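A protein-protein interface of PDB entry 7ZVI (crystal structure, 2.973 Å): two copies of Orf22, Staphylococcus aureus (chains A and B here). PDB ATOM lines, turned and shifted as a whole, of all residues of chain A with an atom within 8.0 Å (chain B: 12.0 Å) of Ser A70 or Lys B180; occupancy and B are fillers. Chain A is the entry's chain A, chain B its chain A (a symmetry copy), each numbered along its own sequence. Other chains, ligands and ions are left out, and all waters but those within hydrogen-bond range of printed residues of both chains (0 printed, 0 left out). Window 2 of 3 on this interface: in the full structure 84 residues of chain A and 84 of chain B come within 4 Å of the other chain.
OG of Ser A68 sits close to OG1 of Thr B183 (3.3 Å).
ND1 of His B181 sits at hydrogen-bond distance from OD2 of Asp A232, 3.1 Å away.
OH of Tyr A240 lies within hydrogen-bond range of O of Leu B177 (2.9 Å).
The backbone carbonyl oxygen of Lys B179 sits close to the backbone carbonyl oxygen of Ser A68.
Printed residues of chain B within 4 Å of Glu A69: Phe B176.
Ser A70 touches just one residue of chain B: Lys B180 (3.4 Å).
No residue of chain B comes within 4 Å of Pro A71.
No residue of chain B comes within 4 Å of Phe A72.
Tyr A73 touches just one residue of chain B: His B181 (3.0 Å).
No residue of chain B comes within 4 Å of Glu A74.
Asn A76 touches none of the printed residues of chain B.
Of chain B, only His B181 (3.1 Å) and Phe B182 (3.7 Å) come within 4 Å of Asp A232.
Of the printed residues of chain B, Arg A236 touches Lys B180 and Phe B182.
Printed residues of chain A within 4 Å of Leu B177: Tyr A240.
Of chain A, only Ser A70 and Arg A236 come within 4 Å of Lys B180.
Lys B185 touches none of the printed residues of chain A.
The nearest printed residue of chain A that does not touch Thr B183 is Glu A69 (5.9 Å).
Of the 15 printed residues of chain A, 7 touch a printed residue of chain B.
Hydrophobic or aromatic side chains of chain A within 4 Å of the printed part of chain B: Tyr A73 and Tyr A240.
Printed residues of chain B that touch a printed residue of chain A: Phe B176, Leu B177, Lys B179, Lys B180, His B181, Phe B182 and Thr B183.
Hydrophobic or aromatic side chains of chain B that line the printed part of chain A: Phe B176, Leu B177, His B181 and Phe B182.
Among the printed residues, 11 pairs touch across the chains.
Among the printed residues, no Asp or Glu carboxylate lies within 4 Å of a Lys or Arg side-chain nitrogen of the other chain.
The side-chain amide nitrogen of Asn A77 is in hydrogen-bond range of the backbone carbonyl oxygen of Tyr A73 (3.1 Å).
The side-chain hydroxyl (OH) of Tyr A240 sits at hydrogen-bond distance from the guanidinium group (NH2) of Arg A236, at 2.9 Å.
The side-chain amino group (NZ) of Lys B179 is in hydrogen-bond range of the backbone carbonyl oxygen (O) of Phe B176 (2.8 Å).
OG1 of Thr B183 lies within hydrogen-bond range of NZ of Lys B179 (3.0 Å).
No position is printed for both chains.
Of the 11 pairs that touch across the chains among the printed residues, none has its exchanged pair printed and touching as well.
Ser A68 touches His B181 (OG to O, 3.8 Å).
CE1 of Phe B176 touches OE1 of Glu A69, 3.6 Å away.
CE of Lys B180 touches OG of Ser A70 (3.4 Å).
His B181 touches Tyr A73.
Phe B182 touches Asp A232 (N to OD2, 3.7 Å).
Lys B180 touches Arg A236.
CG of Arg A236 touches CE2 of Phe B182, 3.1 Å away.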
ATOM      1  N   GLY A  67     -24.347 -30.094  20.584  1.00  0.00           N
ATOM      2  CA  GLY A  67     -24.193 -28.688  20.159  1.00  0.00           C
ATOM      3  C   GLY A  67     -23.761 -28.570  18.708  1.00  0.00           C
ATOM      4  O   GLY A  67     -23.130 -29.515  18.198  1.00  0.00           O
ATOM      5  N   SER A  68     -24.076 -27.431  18.077  1.00  0.00           N
ATOM      6  CA  SER A  68     -23.709 -27.076  16.679  1.00  0.00           C
ATOM      7  C   SER A  68     -22.284 -26.504  16.623  1.00  0.00           C
ATOM      8  O   SER A  68     -21.813 -26.225  15.500  1.00  0.00           O
ATOM      9  CB  SER A  68     -24.715 -26.113  16.090  1.00  0.00           C
ATOM     10  OG  SER A  68     -24.249 -25.571  14.862  1.00  0.00           O
ATOM     11  N   GLU A  69     -21.625 -26.358  17.781  1.00  0.00           N
ATOM     12  CA  GLU A  69     -20.261 -25.772  17.943  1.00  0.00           C
ATOM     13  C   GLU A  69     -19.276 -26.471  16.997  1.00  0.00           C
ATOM     14  O   GLU A  69     -19.541 -27.629  16.624  1.00  0.00           O
ATOM     15  CB  GLU A  69     -19.758 -25.931  19.380  1.00  0.00           C
ATOM     16  CG  GLU A  69     -20.637 -25.289  20.440  1.00  0.00           C
ATOM     17  CD  GLU A  69     -20.468 -25.902  21.821  1.00  0.00           C
ATOM     18  OE1 GLU A  69     -19.334 -25.875  22.343  1.00  0.00           O
ATOM     19  OE2 GLU A  69     -21.465 -26.423  22.361  1.00  0.00           O
ATOM     20  N   SER A  70     -18.167 -25.802  16.662  1.00  0.00           N
ATOM     21  CA  SER A  70     -17.155 -26.264  15.672  1.00  0.00           C
ATOM     22  C   SER A  70     -16.565 -27.614  16.084  1.00  0.00           C
ATOM     23  O   SER A  70     -16.533 -28.533  15.270  1.00  0.00           O
ATOM     24  CB  SER A  70     -16.071 -25.234  15.455  1.00  0.00           C
ATOM     25  OG  SER A  70     -15.487 -25.382  14.168  1.00  0.00           O
ATOM     26  N   PRO A  71     -16.086 -27.793  17.341  1.00  0.00           N
ATOM     27  CA  PRO A  71     -15.457 -29.054  17.747  1.00  0.00           C
ATOM     28  C   PRO A  71     -16.369 -30.278  17.563  1.00  0.00           C
ATOM     29  O   PRO A  71     -15.854 -31.351  17.304  1.00  0.00           O
ATOM     30  CB  PRO A  71     -15.148 -28.851  19.238  1.00  0.00           C
ATOM     31  CG  PRO A  71     -15.081 -27.348  19.402  1.00  0.00           C
ATOM     32  CD  PRO A  71     -16.122 -26.815  18.439  1.00  0.00           C
ATOM     33  N   PHE A  72     -17.686 -30.083  17.700  1.00  0.00           N
ATOM     34  CA  PHE A  72     -18.732 -31.134  17.585  1.00  0.00           C
ATOM     35  C   PHE A  72     -19.347 -31.129  16.179  1.00  0.00           C
ATOM     36  O   PHE A  72     -19.770 -32.208  15.721  1.00  0.00           O
ATOM     37  CB  PHE A  72     -19.795 -30.935  18.669  1.00  0.00           C
ATOM     38  CG  PHE A  72     -19.246 -30.932  20.073  1.00  0.00           C
ATOM     39  CD1 PHE A  72     -19.011 -32.121  20.747  1.00  0.00           C
ATOM     40  CD2 PHE A  72     -18.944 -29.740  20.713  1.00  0.00           C
ATOM     41  CE1 PHE A  72     -18.498 -32.117  22.035  1.00  0.00           C
ATOM     42  CE2 PHE A  72     -18.430 -29.738  22.000  1.00  0.00           C
ATOM     43  CZ  PHE A  72     -18.209 -30.926  22.659  1.00  0.00           C
ATOM     44  N   TYR A  73     -19.400 -29.967  15.518  1.00  0.00           N
ATOM     45  CA  TYR A  73     -19.956 -29.803  14.148  1.00  0.00           C
ATOM     46  C   TYR A  73     -19.412 -30.914  13.243  1.00  0.00           C
ATOM     47  O   TYR A  73     -20.217 -31.587  12.571  1.00  0.00           O
ATOM     48  CB  TYR A  73     -19.629 -28.427  13.562  1.00  0.00           C
ATOM     49  CG  TYR A  73     -20.038 -28.266  12.120  1.00  0.00           C
ATOM     50  CD1 TYR A  73     -21.362 -28.044  11.773  1.00  0.00           C
ATOM     51  CD2 TYR A  73     -19.109 -28.365  11.096  1.00  0.00           C
ATOM     52  CE1 TYR A  73     -21.751 -27.909  10.449  1.00  0.00           C
ATOM     53  CE2 TYR A  73     -19.481 -28.233   9.767  1.00  0.00           C
ATOM     54  CZ  TYR A  73     -20.807 -28.005   9.442  1.00  0.00           C
ATOM     55  OH  TYR A  73     -21.180 -27.878   8.136  1.00  0.00           O
ATOM     56  N   GLU A  74     -18.086 -31.096  13.240  1.00  0.00           N
ATOM     57  CA  GLU A  74     -17.372 -32.104  12.409  1.00  0.00           C
ATOM     58  C   GLU A  74     -17.739 -33.517  12.885  1.00  0.00           C
ATOM     59  O   GLU A  74     -18.031 -34.366  12.018  1.00  0.00           O
ATOM     60  CB  GLU A  74     -15.857 -31.879  12.455  1.00  0.00           C
ATOM     61  CG  GLU A  74     -15.394 -30.670  11.657  1.00  0.00           C
ATOM     62  CD  GLU A  74     -15.260 -29.379  12.448  1.00  0.00           C
ATOM     63  OE1 GLU A  74     -15.880 -28.372  12.050  1.00  0.00           O
ATOM     64  OE2 GLU A  74     -14.519 -29.380  13.452  1.00  0.00           O
ATOM     65  N   ILE A  75     -17.730 -33.754  14.202  1.00  0.00           N
ATOM     66  CA  ILE A  75     -18.072 -35.073  14.823  1.00  0.00           C
ATOM     67  C   ILE A  75     -19.486 -35.477  14.387  1.00  0.00           C
ATOM     68  O   ILE A  75     -19.684 -36.666  14.076  1.00  0.00           O
ATOM     69  CB  ILE A  75     -17.948 -35.029  16.361  1.00  0.00           C
ATOM     70  CG1 ILE A  75     -16.497 -34.836  16.810  1.00  0.00           C
ATOM     71  CG2 ILE A  75     -18.564 -36.272  16.987  1.00  0.00           C
ATOM     72  CD1 ILE A  75     -16.346 -34.548  18.286  1.00  0.00           C
ATOM     73  N   ASN A  76     -20.424 -34.525  14.375  1.00  0.00           N
ATOM     74  CA  ASN A  76     -21.863 -34.759  14.075  1.00  0.00           C
ATOM     75  C   ASN A  76     -22.029 -35.172  12.607  1.00  0.00           C
ATOM     76  O   ASN A  76     -22.635 -36.232  12.364  1.00  0.00           O
ATOM     77  CB  ASN A  76     -22.714 -33.528  14.397  1.00  0.00           C
ATOM     78  CG  ASN A  76     -22.730 -33.188  15.873  1.00  0.00           C
ATOM     79  OD1 ASN A  76     -22.064 -33.839  16.675  1.00  0.00           O
ATOM     80  ND2 ASN A  76     -23.488 -32.168  16.240  1.00  0.00           N
ATOM     81  N   ASN A  77     -21.517 -34.362  11.676  1.00  0.00           N
ATOM     82  CA  ASN A  77     -21.607 -34.600  10.209  1.00  0.00           C
ATOM     83  C   ASN A  77     -20.996 -35.964   9.872  1.00  0.00           C
ATOM     84  O   ASN A  77     -21.625 -36.712   9.099  1.00  0.00           O
ATOM     85  CB  ASN A  77     -20.947 -33.478   9.403  1.00  0.00           C
ATOM     86  CG  ASN A  77     -21.886 -32.316   9.150  1.00  0.00           C
ATOM     87  OD1 ASN A  77     -22.838 -32.441   8.383  1.00  0.00           O
ATOM     88  ND2 ASN A  77     -21.632 -31.185   9.788  1.00  0.00           N
ATOM     89  N   ASP A 232     -24.471 -18.001   4.613  1.00  0.00           N
ATOM     90  CA  ASP A 232     -24.156 -18.112   6.064  1.00  0.00           C
ATOM     91  C   ASP A 232     -23.032 -17.132   6.421  1.00  0.00           C
ATOM     92  O   ASP A 232     -23.224 -16.324   7.348  1.00  0.00           O
ATOM     93  CB  ASP A 232     -23.750 -19.538   6.450  1.00  0.00           C
ATOM     94  CG  ASP A 232     -24.880 -20.555   6.395  1.00  0.00           C
ATOM     95  OD1 ASP A 232     -25.992 -20.181   5.970  1.00  0.00           O
ATOM     96  OD2 ASP A 232     -24.636 -21.716   6.779  1.00  0.00           O
ATOM     97  N   LYS A 233     -21.913 -17.201   5.694  1.00  0.00           N
ATOM     98  CA  LYS A 233     -20.667 -16.441   5.989  1.00  0.00           C
ATOM     99  C   LYS A 233     -20.894 -14.942   5.743  1.00  0.00           C
ATOM    100  O   LYS A 233     -20.169 -14.138   6.363  1.00  0.00           O
ATOM    101  CB  LYS A 233     -19.499 -16.982   5.155  1.00  0.00           C
ATOM    102  CG  LYS A 233     -19.179 -18.461   5.352  1.00  0.00           C
ATOM    103  CD  LYS A 233     -18.817 -18.849   6.775  1.00  0.00           C
ATOM    104  CE  LYS A 233     -17.500 -18.266   7.241  1.00  0.00           C
ATOM    105  NZ  LYS A 233     -17.115 -18.785   8.575  1.00  0.00           N
ATOM    106  N   ARG A 236     -23.280 -13.690   9.043  1.00  0.00           N
ATOM    107  CA  ARG A 236     -22.555 -13.757  10.346  1.00  0.00           C
ATOM    108  C   ARG A 236     -21.869 -12.413  10.605  1.00  0.00           C
ATOM    109  O   ARG A 236     -21.954 -11.921  11.746  1.00  0.00           O
ATOM    110  CB  ARG A 236     -21.503 -14.870  10.357  1.00  0.00           C
ATOM    111  CG  ARG A 236     -22.073 -16.279  10.342  1.00  0.00           C
ATOM    112  CD  ARG A 236     -21.125 -17.323   9.786  1.00  0.00           C
ATOM    113  NE  ARG A 236     -19.726 -16.993  10.027  1.00  0.00           N
ATOM    114  CZ  ARG A 236     -19.104 -17.079  11.202  1.00  0.00           C
ATOM    115  NH1 ARG A 236     -17.827 -16.747  11.290  1.00  0.00           N
ATOM    116  NH2 ARG A 236     -19.749 -17.489  12.283  1.00  0.00           N
ATOM    117  N   TYR A 240     -22.812  -9.726  13.699  1.00  0.00           N
ATOM    118  CA  TYR A 240     -21.720  -9.166  14.539  1.00  0.00           C
ATOM    119  C   TYR A 240     -21.765  -7.632  14.503  1.00  0.00           C
ATOM    120  O   TYR A 240     -21.396  -7.007  15.516  1.00  0.00           O
ATOM    121  CB  TYR A 240     -20.340  -9.662  14.086  1.00  0.00           C
ATOM    122  CG  TYR A 240     -20.128 -11.157  14.103  1.00  0.00           C
ATOM    123  CD1 TYR A 240     -20.828 -11.987  14.967  1.00  0.00           C
ATOM    124  CD2 TYR A 240     -19.193 -11.747  13.264  1.00  0.00           C
ATOM    125  CE1 TYR A 240     -20.621 -13.359  14.982  1.00  0.00           C
ATOM    126  CE2 TYR A 240     -18.973 -13.115  13.269  1.00  0.00           C
ATOM    127  CZ  TYR A 240     -19.689 -13.926  14.130  1.00  0.00           C
ATOM    128  OH  TYR A 240     -19.478 -15.276  14.142  1.00  0.00           O
ATOM    129  N   LEU B 172     -29.435 -14.303  22.090  1.00  0.00           N
ATOM    130  CA  LEU B 172     -28.197 -15.078  21.828  1.00  0.00           C
ATOM    131  C   LEU B 172     -27.847 -15.832  23.114  1.00  0.00           C
ATOM    132  O   LEU B 172     -26.705 -15.704  23.600  1.00  0.00           O
ATOM    133  CB  LEU B 172     -27.084 -14.128  21.373  1.00  0.00           C
ATOM    134  CG  LEU B 172     -27.337 -13.449  20.029  1.00  0.00           C
ATOM    135  CD1 LEU B 172     -26.534 -12.168  19.903  1.00  0.00           C
ATOM    136  CD2 LEU B 172     -27.020 -14.396  18.884  1.00  0.00           C
ATOM    137  N   ASN B 174     -27.299 -18.768  23.360  1.00  0.00           N
ATOM    138  CA  ASN B 174     -26.043 -19.451  22.951  1.00  0.00           C
ATOM    139  C   ASN B 174     -24.956 -18.384  22.785  1.00  0.00           C
ATOM    140  O   ASN B 174     -25.000 -17.650  21.776  1.00  0.00           O
ATOM    141  CB  ASN B 174     -26.216 -20.271  21.668  1.00  0.00           C
ATOM    142  CG  ASN B 174     -26.932 -21.590  21.885  1.00  0.00           C
ATOM    143  OD1 ASN B 174     -27.425 -21.873  22.975  1.00  0.00           O
ATOM    144  ND2 ASN B 174     -26.996 -22.407  20.845  1.00  0.00           N
ATOM    145  N   ASN B 175     -24.035 -18.293  23.751  1.00  0.00           N
ATOM    146  CA  ASN B 175     -22.819 -17.437  23.679  1.00  0.00           C
ATOM    147  C   ASN B 175     -21.903 -17.968  22.571  1.00  0.00           C
ATOM    148  O   ASN B 175     -21.069 -17.188  22.067  1.00  0.00           O
ATOM    149  CB  ASN B 175     -22.086 -17.358  25.024  1.00  0.00           C
ATOM    150  CG  ASN B 175     -22.586 -16.239  25.917  1.00  0.00           C
ATOM    151  OD1 ASN B 175     -22.917 -15.156  25.439  1.00  0.00           O
ATOM    152  ND2 ASN B 175     -22.624 -16.480  27.218  1.00  0.00           N
ATOM    153  N   PHE B 176     -22.062 -19.247  22.211  1.00  0.00           N
ATOM    154  CA  PHE B 176     -21.383 -19.911  21.068  1.00  0.00           C
ATOM    155  C   PHE B 176     -22.062 -19.474  19.763  1.00  0.00           C
ATOM    156  O   PHE B 176     -22.887 -20.243  19.229  1.00  0.00           O
ATOM    157  CB  PHE B 176     -21.410 -21.434  21.234  1.00  0.00           C
ATOM    158  CG  PHE B 176     -20.826 -21.944  22.529  1.00  0.00           C
ATOM    159  CD1 PHE B 176     -19.464 -22.178  22.652  1.00  0.00           C
ATOM    160  CD2 PHE B 176     -21.640 -22.194  23.625  1.00  0.00           C
ATOM    161  CE1 PHE B 176     -18.930 -22.647  23.844  1.00  0.00           C
ATOM    162  CE2 PHE B 176     -21.104 -22.663  24.815  1.00  0.00           C
ATOM    163  CZ  PHE B 176     -19.750 -22.888  24.923  1.00  0.00           C
ATOM    164  N   LEU B 177     -21.740 -18.268  19.282  1.00  0.00           N
ATOM    165  CA  LEU B 177     -22.127 -17.758  17.936  1.00  0.00           C
ATOM    166  C   LEU B 177     -20.884 -17.771  17.035  1.00  0.00           C
ATOM    167  O   LEU B 177     -20.643 -16.779  16.314  1.00  0.00           O
ATOM    168  CB  LEU B 177     -22.731 -16.355  18.072  1.00  0.00           C
ATOM    169  CG  LEU B 177     -23.609 -15.906  16.903  1.00  0.00           C
ATOM    170  CD1 LEU B 177     -24.948 -16.632  16.919  1.00  0.00           C
ATOM    171  CD2 LEU B 177     -23.821 -14.400  16.922  1.00  0.00           C
ATOM    172  N   ASN B 178     -20.132 -18.875  17.086  1.00  0.00           N
ATOM    173  CA  ASN B 178     -18.887 -19.128  16.312  1.00  0.00           C
ATOM    174  C   ASN B 178     -18.884 -20.606  15.902  1.00  0.00           C
ATOM    175  O   ASN B 178     -17.928 -21.323  16.259  1.00  0.00           O
ATOM    176  CB  ASN B 178     -17.644 -18.739  17.119  1.00  0.00           C
ATOM    177  CG  ASN B 178     -17.574 -19.417  18.473  1.00  0.00           C
ATOM    178  OD1 ASN B 178     -18.601 -19.725  19.073  1.00  0.00           O
ATOM    179  ND2 ASN B 178     -16.368 -19.656  18.964  1.00  0.00           N
ATOM    180  N   LYS B 179     -19.927 -21.035  15.182  1.00  0.00           N
ATOM    181  CA  LYS B 179     -20.291 -22.467  14.991  1.00  0.00           C
ATOM    182  C   LYS B 179     -20.305 -22.846  13.502  1.00  0.00           C
ATOM    183  O   LYS B 179     -20.904 -23.894  13.179  1.00  0.00           O
ATOM    184  CB  LYS B 179     -21.663 -22.736  15.621  1.00  0.00           C
ATOM    185  CG  LYS B 179     -22.823 -21.955  15.015  1.00  0.00           C
ATOM    186  CD  LYS B 179     -23.199 -20.698  15.776  1.00  0.00           C
ATOM    187  CE  LYS B 179     -24.469 -20.848  16.589  1.00  0.00           C
ATOM    188  NZ  LYS B 179     -24.372 -21.944  17.584  1.00  0.00           N
ATOM    189  N   LYS B 180     -19.672 -22.045  12.636  1.00  0.00           N
ATOM    190  CA  LYS B 180     -19.586 -22.280  11.167  1.00  0.00           C
ATOM    191  C   LYS B 180     -20.983 -22.098  10.550  1.00  0.00           C
ATOM    192  O   LYS B 180     -21.496 -20.961  10.611  1.00  0.00           O
ATOM    193  CB  LYS B 180     -18.967 -23.655  10.885  1.00  0.00           C
ATOM    194  CG  LYS B 180     -17.591 -23.882  11.495  1.00  0.00           C
ATOM    195  CD  LYS B 180     -16.530 -22.950  10.950  1.00  0.00           C
ATOM    196  CE  LYS B 180     -15.159 -23.193  11.544  1.00  0.00           C
ATOM    197  NZ  LYS B 180     -14.148 -22.279  10.962  1.00  0.00           N
ATOM    198  N   HIS B 181     -21.569 -23.157   9.976  1.00  0.00           N
ATOM    199  CA  HIS B 181     -22.946 -23.165   9.412  1.00  0.00           C
ATOM    200  C   HIS B 181     -23.949 -23.034  10.561  1.00  0.00           C
ATOM    201  O   HIS B 181     -23.868 -23.846  11.506  1.00  0.00           O
ATOM    202  CB  HIS B 181     -23.184 -24.424   8.569  1.00  0.00           C
ATOM    203  CG  HIS B 181     -22.293 -24.521   7.375  1.00  0.00           C
ATOM    204  ND1 HIS B 181     -22.667 -24.051   6.130  1.00  0.00           N
ATOM    205  CD2 HIS B 181     -21.046 -25.024   7.232  1.00  0.00           C
ATOM    206  CE1 HIS B 181     -21.691 -24.265   5.271  1.00  0.00           C
ATOM    207  NE2 HIS B 181     -20.685 -24.861   5.922  1.00  0.00           N
ATOM    208  N   PHE B 182     -24.852 -22.051  10.475  1.00  0.00           N
ATOM    209  CA  PHE B 182     -25.716 -21.583  11.592  1.00  0.00           C
ATOM    210  C   PHE B 182     -26.697 -22.682  12.011  1.00  0.00           C
ATOM    211  O   PHE B 182     -27.444 -23.186  11.143  1.00  0.00           O
ATOM    212  CB  PHE B 182     -26.462 -20.299  11.221  1.00  0.00           C
ATOM    213  CG  PHE B 182     -25.780 -19.038  11.685  1.00  0.00           C
ATOM    214  CD1 PHE B 182     -25.346 -18.911  12.997  1.00  0.00           C
ATOM    215  CD2 PHE B 182     -25.582 -17.975  10.819  1.00  0.00           C
ATOM    216  CE1 PHE B 182     -24.719 -17.753  13.430  1.00  0.00           C
ATOM    217  CE2 PHE B 182     -24.966 -16.813  11.257  1.00  0.00           C
ATOM    218  CZ  PHE B 182     -24.532 -16.706  12.559  1.00  0.00           C
ATOM    219  N   THR B 183     -26.697 -23.009  13.312  1.00  0.00           N
ATOM    220  CA  THR B 183     -27.535 -24.064  13.946  1.00  0.00           C
ATOM    221  C   THR B 183     -28.865 -24.171  13.192  1.00  0.00           C
ATOM    222  O   THR B 183     -29.612 -23.171  13.163  1.00  0.00           O
ATOM    223  CB  THR B 183     -27.758 -23.789  15.440  1.00  0.00           C
ATOM    224  OG1 THR B 183     -26.503 -23.463  16.040  1.00  0.00           O
ATOM    225  CG2 THR B 183     -28.380 -24.965  16.161  1.00  0.00           C
ATOM    226  N   GLU B 184     -29.124 -25.338  12.594  1.00  0.00           N
ATOM    227  CA  GLU B 184     -30.323 -25.632  11.763  1.00  0.00           C
ATOM    228  C   GLU B 184     -31.570 -25.054  12.439  1.00  0.00           C
ATOM    229  O   GLU B 184     -31.850 -25.443  13.591  1.00  0.00           O
ATOM    230  CB  GLU B 184     -30.464 -27.144  11.559  1.00  0.00           C
ATOM    231  CG  GLU B 184     -31.679 -27.548  10.738  1.00  0.00           C
ATOM    232  CD  GLU B 184     -32.927 -27.939  11.516  1.00  0.00           C
ATOM    233  OE1 GLU B 184     -32.797 -28.383  12.676  1.00  0.00           O
ATOM    234  OE2 GLU B 184     -34.033 -27.808  10.951  1.00  0.00           O
ATOM    235  N   LYS B 185     -32.272 -24.143  11.756  1.00  0.00           N
ATOM    236  CA  LYS B 185     -33.590 -23.598  12.177  1.00  0.00           C
ATOM    237  C   LYS B 185     -33.519 -22.993  13.588  1.00  0.00           C
ATOM    238  O   LYS B 185     -34.590 -22.787  14.188  1.00  0.00           O
ATOM    239  CB  LYS B 185     -34.648 -24.704  12.121  1.00  0.00           C
ATOM    240  CG  LYS B 185     -35.406 -24.811  10.805  1.00  0.00           C
ATOM    241  CD  LYS B 185     -36.797 -25.405  10.939  1.00  0.00           C
ATOM    242  CE  LYS B 185     -37.682 -24.711  11.957  1.00  0.00           C
ATOM    243  NZ  LYS B 185     -37.515 -23.237  11.959  1.00  0.00           N
ATOM    244  N   ASP B 186     -32.314 -22.713  14.096  1.00  0.00           N
ATOM    245  CA  ASP B 186     -32.092 -21.965  15.364  1.00  0.00           C
ATOM    246  C   ASP B 186     -31.492 -20.598  15.007  1.00  0.00           C
ATOM    247  O   ASP B 186     -30.835 -19.984  15.867  1.00  0.00           O
ATOM    248  CB  ASP B 186     -31.264 -22.796  16.346  1.00  0.00           C
ATOM    249  CG  ASP B 186     -32.002 -24.022  16.865  1.00  0.00           C
ATOM    250  OD1 ASP B 186     -33.147 -24.253  16.424  1.00  0.00           O
ATOM    251  OD2 ASP B 186     -31.425 -24.739  17.706  1.00  0.00           O
ATOM    252  N   MET B 187     -31.709 -20.173  13.758  1.00  0.00           N
ATOM    253  CA  MET B 187     -31.694 -18.757  13.305  1.00  0.00           C
ATOM    254  C   MET B 187     -33.083 -18.143  13.535  1.00  0.00           C
ATOM    255  O   MET B 187     -33.228 -16.924  13.325  1.00  0.00           O
ATOM    256  CB  MET B 187     -31.318 -18.654  11.821  1.00  0.00           C
ATOM    257  CG  MET B 187     -32.295 -19.345  10.877  1.00  0.00           C
ATOM    258  SD  MET B 187     -31.508 -19.998   9.376  1.00  0.00           S
ATOM    259  CE  MET B 187     -30.473 -21.285  10.071  1.00  0.00           C
